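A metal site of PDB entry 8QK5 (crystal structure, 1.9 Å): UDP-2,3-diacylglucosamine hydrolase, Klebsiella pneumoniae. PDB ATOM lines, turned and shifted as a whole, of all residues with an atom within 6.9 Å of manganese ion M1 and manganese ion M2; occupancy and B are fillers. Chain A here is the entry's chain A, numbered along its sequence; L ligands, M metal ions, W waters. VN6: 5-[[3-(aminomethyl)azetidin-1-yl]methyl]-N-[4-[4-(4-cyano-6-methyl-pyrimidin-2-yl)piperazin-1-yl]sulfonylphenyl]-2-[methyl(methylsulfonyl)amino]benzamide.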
ATOM      1  N   ALA A   7     -10.610   9.468 -29.327  1.00  0.00           N
ATOM      2  CA  ALA A   7      -9.574   9.404 -28.310  1.00  0.00           C
ATOM      3  C   ALA A   7      -8.221   9.491 -29.011  1.00  0.00           C
ATOM      4  O   ALA A   7      -8.117   9.318 -30.225  1.00  0.00           O
ATOM      5  CB  ALA A   7      -9.732   8.151 -27.492  1.00  0.00           C
ATOM      6  N   ASP A   8      -7.184   9.815 -28.233  1.00  0.00           N
ATOM      7  CA  ASP A   8      -5.832   9.595 -28.696  1.00  0.00           C
ATOM      8  C   ASP A   8      -5.542  10.501 -29.882  1.00  0.00           C
ATOM      9  O   ASP A   8      -4.836  10.110 -30.816  1.00  0.00           O
ATOM     10  CB  ASP A   8      -5.600   8.106 -28.979  1.00  0.00           C
ATOM     11  CG  ASP A   8      -5.691   7.264 -27.722  1.00  0.00           C
ATOM     12  OD1 ASP A   8      -4.876   7.491 -26.801  1.00  0.00           O
ATOM     13  OD2 ASP A   8      -6.577   6.387 -27.653  1.00  0.00           O
ATOM     14  N   LEU A   9      -6.037  11.735 -29.800  1.00  0.00           N
ATOM     15  CA  LEU A   9      -5.675  12.763 -30.762  1.00  0.00           C
ATOM     16  C   LEU A   9      -4.232  13.263 -30.556  1.00  0.00           C
ATOM     17  O   LEU A   9      -3.586  13.685 -31.511  1.00  0.00           O
ATOM     18  CB  LEU A   9      -6.689  13.910 -30.664  1.00  0.00           C
ATOM     19  CG  LEU A   9      -8.100  13.538 -31.108  1.00  0.00           C
ATOM     20  CD1 LEU A   9      -8.955  13.119 -29.939  1.00  0.00           C
ATOM     21  CD2 LEU A   9      -8.740  14.693 -31.823  1.00  0.00           C
ATOM     22  N   HIS A  10      -3.736  13.274 -29.317  1.00  0.00           N
ATOM     23  CA  HIS A  10      -2.366  13.715 -29.053  1.00  0.00           C
ATOM     24  C   HIS A  10      -2.091  15.112 -29.626  1.00  0.00           C
ATOM     25  O   HIS A  10      -1.052  15.357 -30.241  1.00  0.00           O
ATOM     26  CB  HIS A  10      -1.367  12.658 -29.547  1.00  0.00           C
ATOM     27  CG  HIS A  10      -1.531  11.368 -28.816  1.00  0.00           C
ATOM     28  ND1 HIS A  10      -1.035  11.232 -27.543  1.00  0.00           N
ATOM     29  CD2 HIS A  10      -2.166  10.240 -29.078  1.00  0.00           C
ATOM     30  CE1 HIS A  10      -1.361  10.041 -27.065  1.00  0.00           C
ATOM     31  NE2 HIS A  10      -2.069   9.423 -27.971  1.00  0.00           N
ATOM     32  N   LEU A  39     -12.342  10.158 -25.142  1.00  0.00           N
ATOM     33  CA  LEU A  39     -11.903   9.213 -24.127  1.00  0.00           C
ATOM     34  C   LEU A  39     -10.392   9.298 -23.907  1.00  0.00           C
ATOM     35  O   LEU A  39      -9.716   8.278 -23.873  1.00  0.00           O
ATOM     36  CB  LEU A  39     -12.314   7.812 -24.566  1.00  0.00           C
ATOM     37  CG  LEU A  39     -13.776   7.667 -24.946  1.00  0.00           C
ATOM     38  CD1 LEU A  39     -14.083   6.187 -25.153  1.00  0.00           C
ATOM     39  CD2 LEU A  39     -14.688   8.272 -23.890  1.00  0.00           C
ATOM     40  N   GLY A  40      -9.881  10.535 -23.751  1.00  0.00           N
ATOM     41  CA  GLY A  40      -8.544  10.768 -23.227  1.00  0.00           C
ATOM     42  C   GLY A  40      -7.502  10.938 -24.326  1.00  0.00           C
ATOM     43  O   GLY A  40      -7.743  10.605 -25.493  1.00  0.00           O
ATOM     44  N   ASP A  41      -6.356  11.477 -23.937  1.00  0.00           N
ATOM     45  CA  ASP A  41      -5.269  11.782 -24.834  1.00  0.00           C
ATOM     46  C   ASP A  41      -5.778  12.716 -25.923  1.00  0.00           C
ATOM     47  O   ASP A  41      -5.399  12.598 -27.102  1.00  0.00           O
ATOM     48  CB  ASP A  41      -4.587  10.520 -25.369  1.00  0.00           C
ATOM     49  CG  ASP A  41      -3.740   9.819 -24.327  1.00  0.00           C
ATOM     50  OD1 ASP A  41      -3.797  10.262 -23.148  1.00  0.00           O
ATOM     51  OD2 ASP A  41      -3.062   8.823 -24.670  1.00  0.00           O
ATOM     52  N   GLU A  44      -1.200  15.768 -26.272  1.00  0.00           N
ATOM     53  CA  GLU A  44       0.027  14.995 -26.161  1.00  0.00           C
ATOM     54  C   GLU A  44       0.619  15.133 -24.769  1.00  0.00           C
ATOM     55  O   GLU A  44       1.316  14.242 -24.304  1.00  0.00           O
ATOM     56  CB  GLU A  44       1.027  15.466 -27.221  1.00  0.00           C
ATOM     57  CG  GLU A  44       2.406  14.823 -27.163  1.00  0.00           C
ATOM     58  CD  GLU A  44       2.521  13.305 -27.107  1.00  0.00           C
ATOM     59  OE1 GLU A  44       1.505  12.591 -27.273  1.00  0.00           O
ATOM     60  OE2 GLU A  44       3.626  12.826 -26.869  1.00  0.00           O
ATOM     61  N   GLY A  78      -6.866  10.660 -20.318  1.00  0.00           N
ATOM     62  CA  GLY A  78      -5.907   9.634 -20.648  1.00  0.00           C
ATOM     63  C   GLY A  78      -4.642   9.732 -19.789  1.00  0.00           C
ATOM     64  O   GLY A  78      -4.607  10.423 -18.779  1.00  0.00           O
ATOM     65  N   ASN A  79      -3.635   8.974 -20.176  1.00  0.00           N
ATOM     66  CA  ASN A  79      -2.387   8.891 -19.440  1.00  0.00           C
ATOM     67  C   ASN A  79      -1.572  10.140 -19.716  1.00  0.00           C
ATOM     68  O   ASN A  79      -0.713  10.485 -18.922  1.00  0.00           O
ATOM     69  CB  ASN A  79      -1.593   7.635 -19.787  1.00  0.00           C
ATOM     70  CG  ASN A  79      -1.174   7.582 -21.245  1.00  0.00           C
ATOM     71  OD1 ASN A  79      -2.035   7.454 -22.087  1.00  0.00           O
ATOM     72  ND2 ASN A  79       0.099   7.700 -21.569  1.00  0.00           N
ATOM     73  N   ARG A  80      -1.851  10.806 -20.846  1.00  0.00           N
ATOM     74  CA  ARG A  80      -1.070  11.963 -21.260  1.00  0.00           C
ATOM     75  C   ARG A  80      -1.618  13.236 -20.618  1.00  0.00           C
ATOM     76  O   ARG A  80      -0.829  14.141 -20.347  1.00  0.00           O
ATOM     77  CB  ARG A  80      -1.002  12.161 -22.778  1.00  0.00           C
ATOM     78  CG  ARG A  80      -0.420  10.986 -23.576  1.00  0.00           C
ATOM     79  CD  ARG A  80       0.994  10.605 -23.223  1.00  0.00           C
ATOM     80  NE  ARG A  80       1.917  11.704 -23.467  1.00  0.00           N
ATOM     81  CZ  ARG A  80       3.224  11.650 -23.252  1.00  0.00           C
ATOM     82  NH1 ARG A  80       3.792  10.541 -22.825  1.00  0.00           N
ATOM     83  NH2 ARG A  80       3.959  12.730 -23.450  1.00  0.00           N
ATOM     84  N   HIS A 114     -10.676   5.302 -20.887  1.00  0.00           N
ATOM     85  CA  HIS A 114      -9.487   5.555 -21.696  1.00  0.00           C
ATOM     86  C   HIS A 114      -8.892   4.222 -22.127  1.00  0.00           C
ATOM     87  O   HIS A 114      -8.560   4.050 -23.287  1.00  0.00           O
ATOM     88  CB  HIS A 114      -8.430   6.382 -20.959  1.00  0.00           C
ATOM     89  CG  HIS A 114      -7.243   6.631 -21.831  1.00  0.00           C
ATOM     90  ND1 HIS A 114      -7.405   7.261 -23.045  1.00  0.00           N
ATOM     91  CD2 HIS A 114      -5.922   6.369 -21.709  1.00  0.00           C
ATOM     92  CE1 HIS A 114      -6.203   7.394 -23.608  1.00  0.00           C
ATOM     93  NE2 HIS A 114      -5.281   6.866 -22.822  1.00  0.00           N
ATOM     94  N   ASP A 116      -6.212   2.666 -20.288  1.00  0.00           N
ATOM     95  CA  ASP A 116      -4.920   2.437 -19.657  1.00  0.00           C
ATOM     96  C   ASP A 116      -5.070   1.547 -18.418  1.00  0.00           C
ATOM     97  O   ASP A 116      -4.159   0.780 -18.090  1.00  0.00           O
ATOM     98  CB  ASP A 116      -4.241   3.761 -19.354  1.00  0.00           C
ATOM     99  CG  ASP A 116      -4.971   4.651 -18.352  1.00  0.00           C
ATOM    100  OD1 ASP A 116      -6.192   4.911 -18.527  1.00  0.00           O
ATOM    101  OD2 ASP A 116      -4.297   5.117 -17.432  1.00  0.00           O
ATOM    102  N   TYR A 125       3.996   1.288 -15.850  1.00  0.00           N
ATOM    103  CA  TYR A 125       3.045   2.346 -16.089  1.00  0.00           C
ATOM    104  C   TYR A 125       2.105   2.493 -14.888  1.00  0.00           C
ATOM    105  O   TYR A 125       1.725   3.608 -14.551  1.00  0.00           O
ATOM    106  CB  TYR A 125       2.241   2.127 -17.371  1.00  0.00           C
ATOM    107  CG  TYR A 125       1.110   3.111 -17.456  1.00  0.00           C
ATOM    108  CD1 TYR A 125       1.363   4.462 -17.638  1.00  0.00           C
ATOM    109  CD2 TYR A 125      -0.188   2.727 -17.209  1.00  0.00           C
ATOM    110  CE1 TYR A 125       0.351   5.407 -17.638  1.00  0.00           C
ATOM    111  CE2 TYR A 125      -1.220   3.649 -17.195  1.00  0.00           C
ATOM    112  CZ  TYR A 125      -0.943   4.997 -17.406  1.00  0.00           C
ATOM    113  OH  TYR A 125      -1.953   5.920 -17.368  1.00  0.00           O
ATOM    114  N   ILE A 171       3.017   0.965 -26.746  1.00  0.00           N
ATOM    115  CA  ILE A 171       2.063   1.034 -25.656  1.00  0.00           C
ATOM    116  C   ILE A 171       1.576  -0.398 -25.357  1.00  0.00           C
ATOM    117  O   ILE A 171       1.119  -1.111 -26.259  1.00  0.00           O
ATOM    118  CB  ILE A 171       0.950   2.050 -25.996  1.00  0.00           C
ATOM    119  CG1 ILE A 171       1.561   3.440 -26.223  1.00  0.00           C
ATOM    120  CG2 ILE A 171      -0.145   2.069 -24.941  1.00  0.00           C
ATOM    121  CD1 ILE A 171       0.576   4.554 -26.412  1.00  0.00           C
ATOM    122  N   GLY A 194      -9.697   3.597 -25.716  1.00  0.00           N
ATOM    123  CA  GLY A 194      -8.613   4.020 -26.577  1.00  0.00           C
ATOM    124  C   GLY A 194      -7.317   3.499 -26.003  1.00  0.00           C
ATOM    125  O   GLY A 194      -7.195   2.326 -25.654  1.00  0.00           O
ATOM    126  N   HIS A 195      -6.390   4.437 -25.803  1.00  0.00           N
ATOM    127  CA  HIS A 195      -5.118   4.211 -25.133  1.00  0.00           C
ATOM    128  C   HIS A 195      -4.138   3.352 -25.946  1.00  0.00           C
ATOM    129  O   HIS A 195      -2.975   3.726 -26.088  1.00  0.00           O
ATOM    130  CB  HIS A 195      -5.290   3.605 -23.748  1.00  0.00           C
ATOM    131  CG  HIS A 195      -3.947   3.533 -23.093  1.00  0.00           C
ATOM    132  ND1 HIS A 195      -3.128   4.634 -22.914  1.00  0.00           N
ATOM    133  CD2 HIS A 195      -3.247   2.452 -22.715  1.00  0.00           C
ATOM    134  CE1 HIS A 195      -2.016   4.218 -22.311  1.00  0.00           C
ATOM    135  NE2 HIS A 195      -2.051   2.900 -22.215  1.00  0.00           N
ATOM    136  N   THR A 196      -4.585   2.197 -26.439  1.00  0.00           N
ATOM    137  CA  THR A 196      -3.685   1.234 -27.049  1.00  0.00           C
ATOM    138  C   THR A 196      -3.253   1.577 -28.474  1.00  0.00           C
ATOM    139  O   THR A 196      -2.304   0.961 -28.973  1.00  0.00           O
ATOM    140  CB  THR A 196      -4.268  -0.184 -27.056  1.00  0.00           C
ATOM    141  OG1 THR A 196      -5.461  -0.191 -27.832  1.00  0.00           O
ATOM    142  CG2 THR A 196      -4.567  -0.730 -25.677  1.00  0.00           C
ATOM    143  N   HIS A 197      -3.980   2.474 -29.151  1.00  0.00           N
ATOM    144  CA  HIS A 197      -3.697   2.868 -30.533  1.00  0.00           C
ATOM    145  C   HIS A 197      -3.739   1.667 -31.487  1.00  0.00           C
ATOM    146  O   HIS A 197      -3.060   1.688 -32.511  1.00  0.00           O
ATOM    147  CB  HIS A 197      -2.339   3.559 -30.646  1.00  0.00           C
ATOM    148  CG  HIS A 197      -2.160   4.727 -29.729  1.00  0.00           C
ATOM    149  ND1 HIS A 197      -0.949   5.376 -29.590  1.00  0.00           N
ATOM    150  CD2 HIS A 197      -3.017   5.346 -28.899  1.00  0.00           C
ATOM    151  CE1 HIS A 197      -1.078   6.337 -28.685  1.00  0.00           C
ATOM    152  NE2 HIS A 197      -2.323   6.347 -28.260  1.00  0.00           N
ATOM    153  N   ALA A 218      -5.348   6.159 -32.700  1.00  0.00           N
ATOM    154  CA  ALA A 218      -4.696   7.453 -32.582  1.00  0.00           C
ATOM    155  C   ALA A 218      -4.839   8.252 -33.876  1.00  0.00           C
ATOM    156  O   ALA A 218      -4.925   7.665 -34.954  1.00  0.00           O
ATOM    157  CB  ALA A 218      -3.239   7.278 -32.207  1.00  0.00           C
HETATM  158  C5  VN6 L   1       2.697  15.188 -11.783  1.00  0.00           C
HETATM  159  C6  VN6 L   1       3.939  15.077 -11.206  1.00  0.00           C
HETATM  160  N7  VN6 L   1       3.630  15.422 -15.257  1.00  0.00           N
HETATM  161  C8  VN6 L   1       2.344  15.882 -15.778  1.00  0.00           C
HETATM  162  C26 VN6 L   1       4.734   6.425 -18.338  1.00  0.00           C
HETATM  163  C27 VN6 L   1       5.284   5.135 -18.255  1.00  0.00           C
HETATM  164  C28 VN6 L   1       4.980   4.183 -19.222  1.00  0.00           C
HETATM  165  C29 VN6 L   1       4.132   4.495 -20.279  1.00  0.00           C
HETATM  166  C30 VN6 L   1       3.593   5.765 -20.401  1.00  0.00           C
HETATM  167  C32 VN6 L   1       2.008   4.797 -21.948  1.00  0.00           C
HETATM  168  C37 VN6 L   1       1.415  15.151 -10.940  1.00  0.00           C
HETATM  169  C38 VN6 L   1       6.362  14.958 -11.446  1.00  0.00           C
HETATM  170  C40 VN6 L   1       6.164   4.707 -17.127  1.00  0.00           C
HETATM  171  C42 VN6 L   1       8.126   4.886 -15.845  1.00  0.00           C
HETATM  172  C1  VN6 L   1       5.066  15.089 -12.003  1.00  0.00           C
HETATM  173  N2  VN6 L   1       4.946  15.231 -13.320  1.00  0.00           N
HETATM  174  C3  VN6 L   1       3.733  15.419 -13.876  1.00  0.00           C
HETATM  175  N4  VN6 L   1       2.609  15.334 -13.120  1.00  0.00           N
HETATM  176  C9  VN6 L   1       2.210  15.248 -17.163  1.00  0.00           C
HETATM  177  C10 VN6 L   1       4.724  15.998 -15.944  1.00  0.00           C
HETATM  178  C11 VN6 L   1       4.699  15.414 -17.378  1.00  0.00           C
HETATM  179  N12 VN6 L   1       3.350  15.697 -18.017  1.00  0.00           N
HETATM  180  S13 VN6 L   1       3.246  15.071 -19.557  1.00  0.00           S
HETATM  181  C14 VN6 L   1       3.457  13.337 -19.525  1.00  0.00           C
HETATM  182  O15 VN6 L   1       1.966  15.425 -20.093  1.00  0.00           O
HETATM  183  O16 VN6 L   1       4.293  15.658 -20.324  1.00  0.00           O
HETATM  184  C17 VN6 L   1       4.714  12.831 -19.676  1.00  0.00           C
HETATM  185  C18 VN6 L   1       4.923  11.477 -19.651  1.00  0.00           C
HETATM  186  C19 VN6 L   1       3.878  10.581 -19.460  1.00  0.00           C
HETATM  187  C20 VN6 L   1       2.356  12.451 -19.306  1.00  0.00           C
HETATM  188  C21 VN6 L   1       2.597  11.057 -19.264  1.00  0.00           C
HETATM  189  N22 VN6 L   1       4.194   9.216 -19.365  1.00  0.00           N
HETATM  190  C23 VN6 L   1       3.306   8.179 -19.504  1.00  0.00           C
HETATM  191  O24 VN6 L   1       2.106   8.392 -19.713  1.00  0.00           O
HETATM  192  C25 VN6 L   1       3.865   6.737 -19.389  1.00  0.00           C
HETATM  193  N31 VN6 L   1       2.668   6.061 -21.477  1.00  0.00           N
HETATM  194  S33 VN6 L   1       3.421   6.796 -22.724  1.00  0.00           S
HETATM  195  C34 VN6 L   1       4.556   5.658 -23.503  1.00  0.00           C
HETATM  196  O35 VN6 L   1       2.415   7.227 -23.643  1.00  0.00           O
HETATM  197  O36 VN6 L   1       4.138   7.948 -22.253  1.00  0.00           O
HETATM  198  N39 VN6 L   1       7.399  14.848 -11.026  1.00  0.00           N
HETATM  199  N41 VN6 L   1       7.326   5.535 -16.940  1.00  0.00           N
HETATM  200  C43 VN6 L   1       8.381   5.198 -17.936  1.00  0.00           C
HETATM  201  C44 VN6 L   1       9.331   4.915 -16.781  1.00  0.00           C
HETATM  202  C45 VN6 L   1      10.145   6.175 -16.475  1.00  0.00           C
HETATM  203  N46 VN6 L   1      11.506   5.817 -16.040  1.00  0.00           N
HETATM  204 MN    MN M   1      -2.763   7.789 -26.608  1.00  0.00          MN
HETATM  205 MN    MN M   2      -3.190   6.801 -23.753  1.00  0.00          MN
HETATM  206  O   HOH W   1      -1.959   6.163 -25.484  1.00  0.00           O
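Within 4 Å of manganese ion M1: Asp 8, His 10, Asp 41 and His 197.
Manganese ion M2 is bound by the side-chain amide oxygen (OD1) of Asn 79, 2.1 Å away. Manganese ion M2 is bound by water W1. The side-chain carboxylate (OD2) of Asp 41 binds manganese ion M2. A ring nitrogen (NE2) of His 114 is bound to manganese ion M2, at 2.3 Å. Manganese ion M2 is bound by ND1 of His 195, 2.3 Å away. Manganese ion M2 has five donor atoms within binding distance.
Of the 20 residues printed, 5 come within 4 Å of manganese ion M2. Along chain A the residues within 4 Å of manganese ion M2 span positions 8 to 195. The nearest printed residue that does not touch manganese ion M2 is His 197 (4.6 Å).
The side-chain carboxylate of Asp 8 lies within hydrogen-bond range of the backbone NH of His 195, 2.7 Å away. The backbone NH (N) of Asp 8 lies within hydrogen-bond range of the backbone carbonyl oxygen (O) of Gly 40, at 2.9 Å. The backbone NH of Arg 80 lies within hydrogen-bond range of the side-chain carboxylate of Asp 41. N of Leu 9 lies within hydrogen-bond range of O of Asp 41. NE2 of His 197 lies close to O of His 195 (3.5 Å). ND1 of His 10 lies within hydrogen-bond range of OE1 of Glu 44, at 2.9 Å. The backbone NH (N) of Gly 194 is in hydrogen-bond range of the backbone carbonyl oxygen (O) of His 114 (2.7 Å). The backbone carbonyl oxygen (O) of Leu 39 sits at hydrogen-bond distance from a ring nitrogen (ND1) of His 114.
Manganese ion M1 is bound by water W1, the side-chain carboxylate of Asp 8, the side-chain carboxylate of Asp 41, a ring nitrogen (NE2) of His 197 and a ring nitrogen (NE2) of His 10. Manganese ion M1 has five donor atoms within binding distance.
The side-chain amide nitrogen (ND2) of Asn 79 is in hydrogen-bond range of an oxygen (O24) of the ligand, 2.8 Å away. O36 of the ligand sits at hydrogen-bond distance from NH1 of Arg 80, 2.7 Å away.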
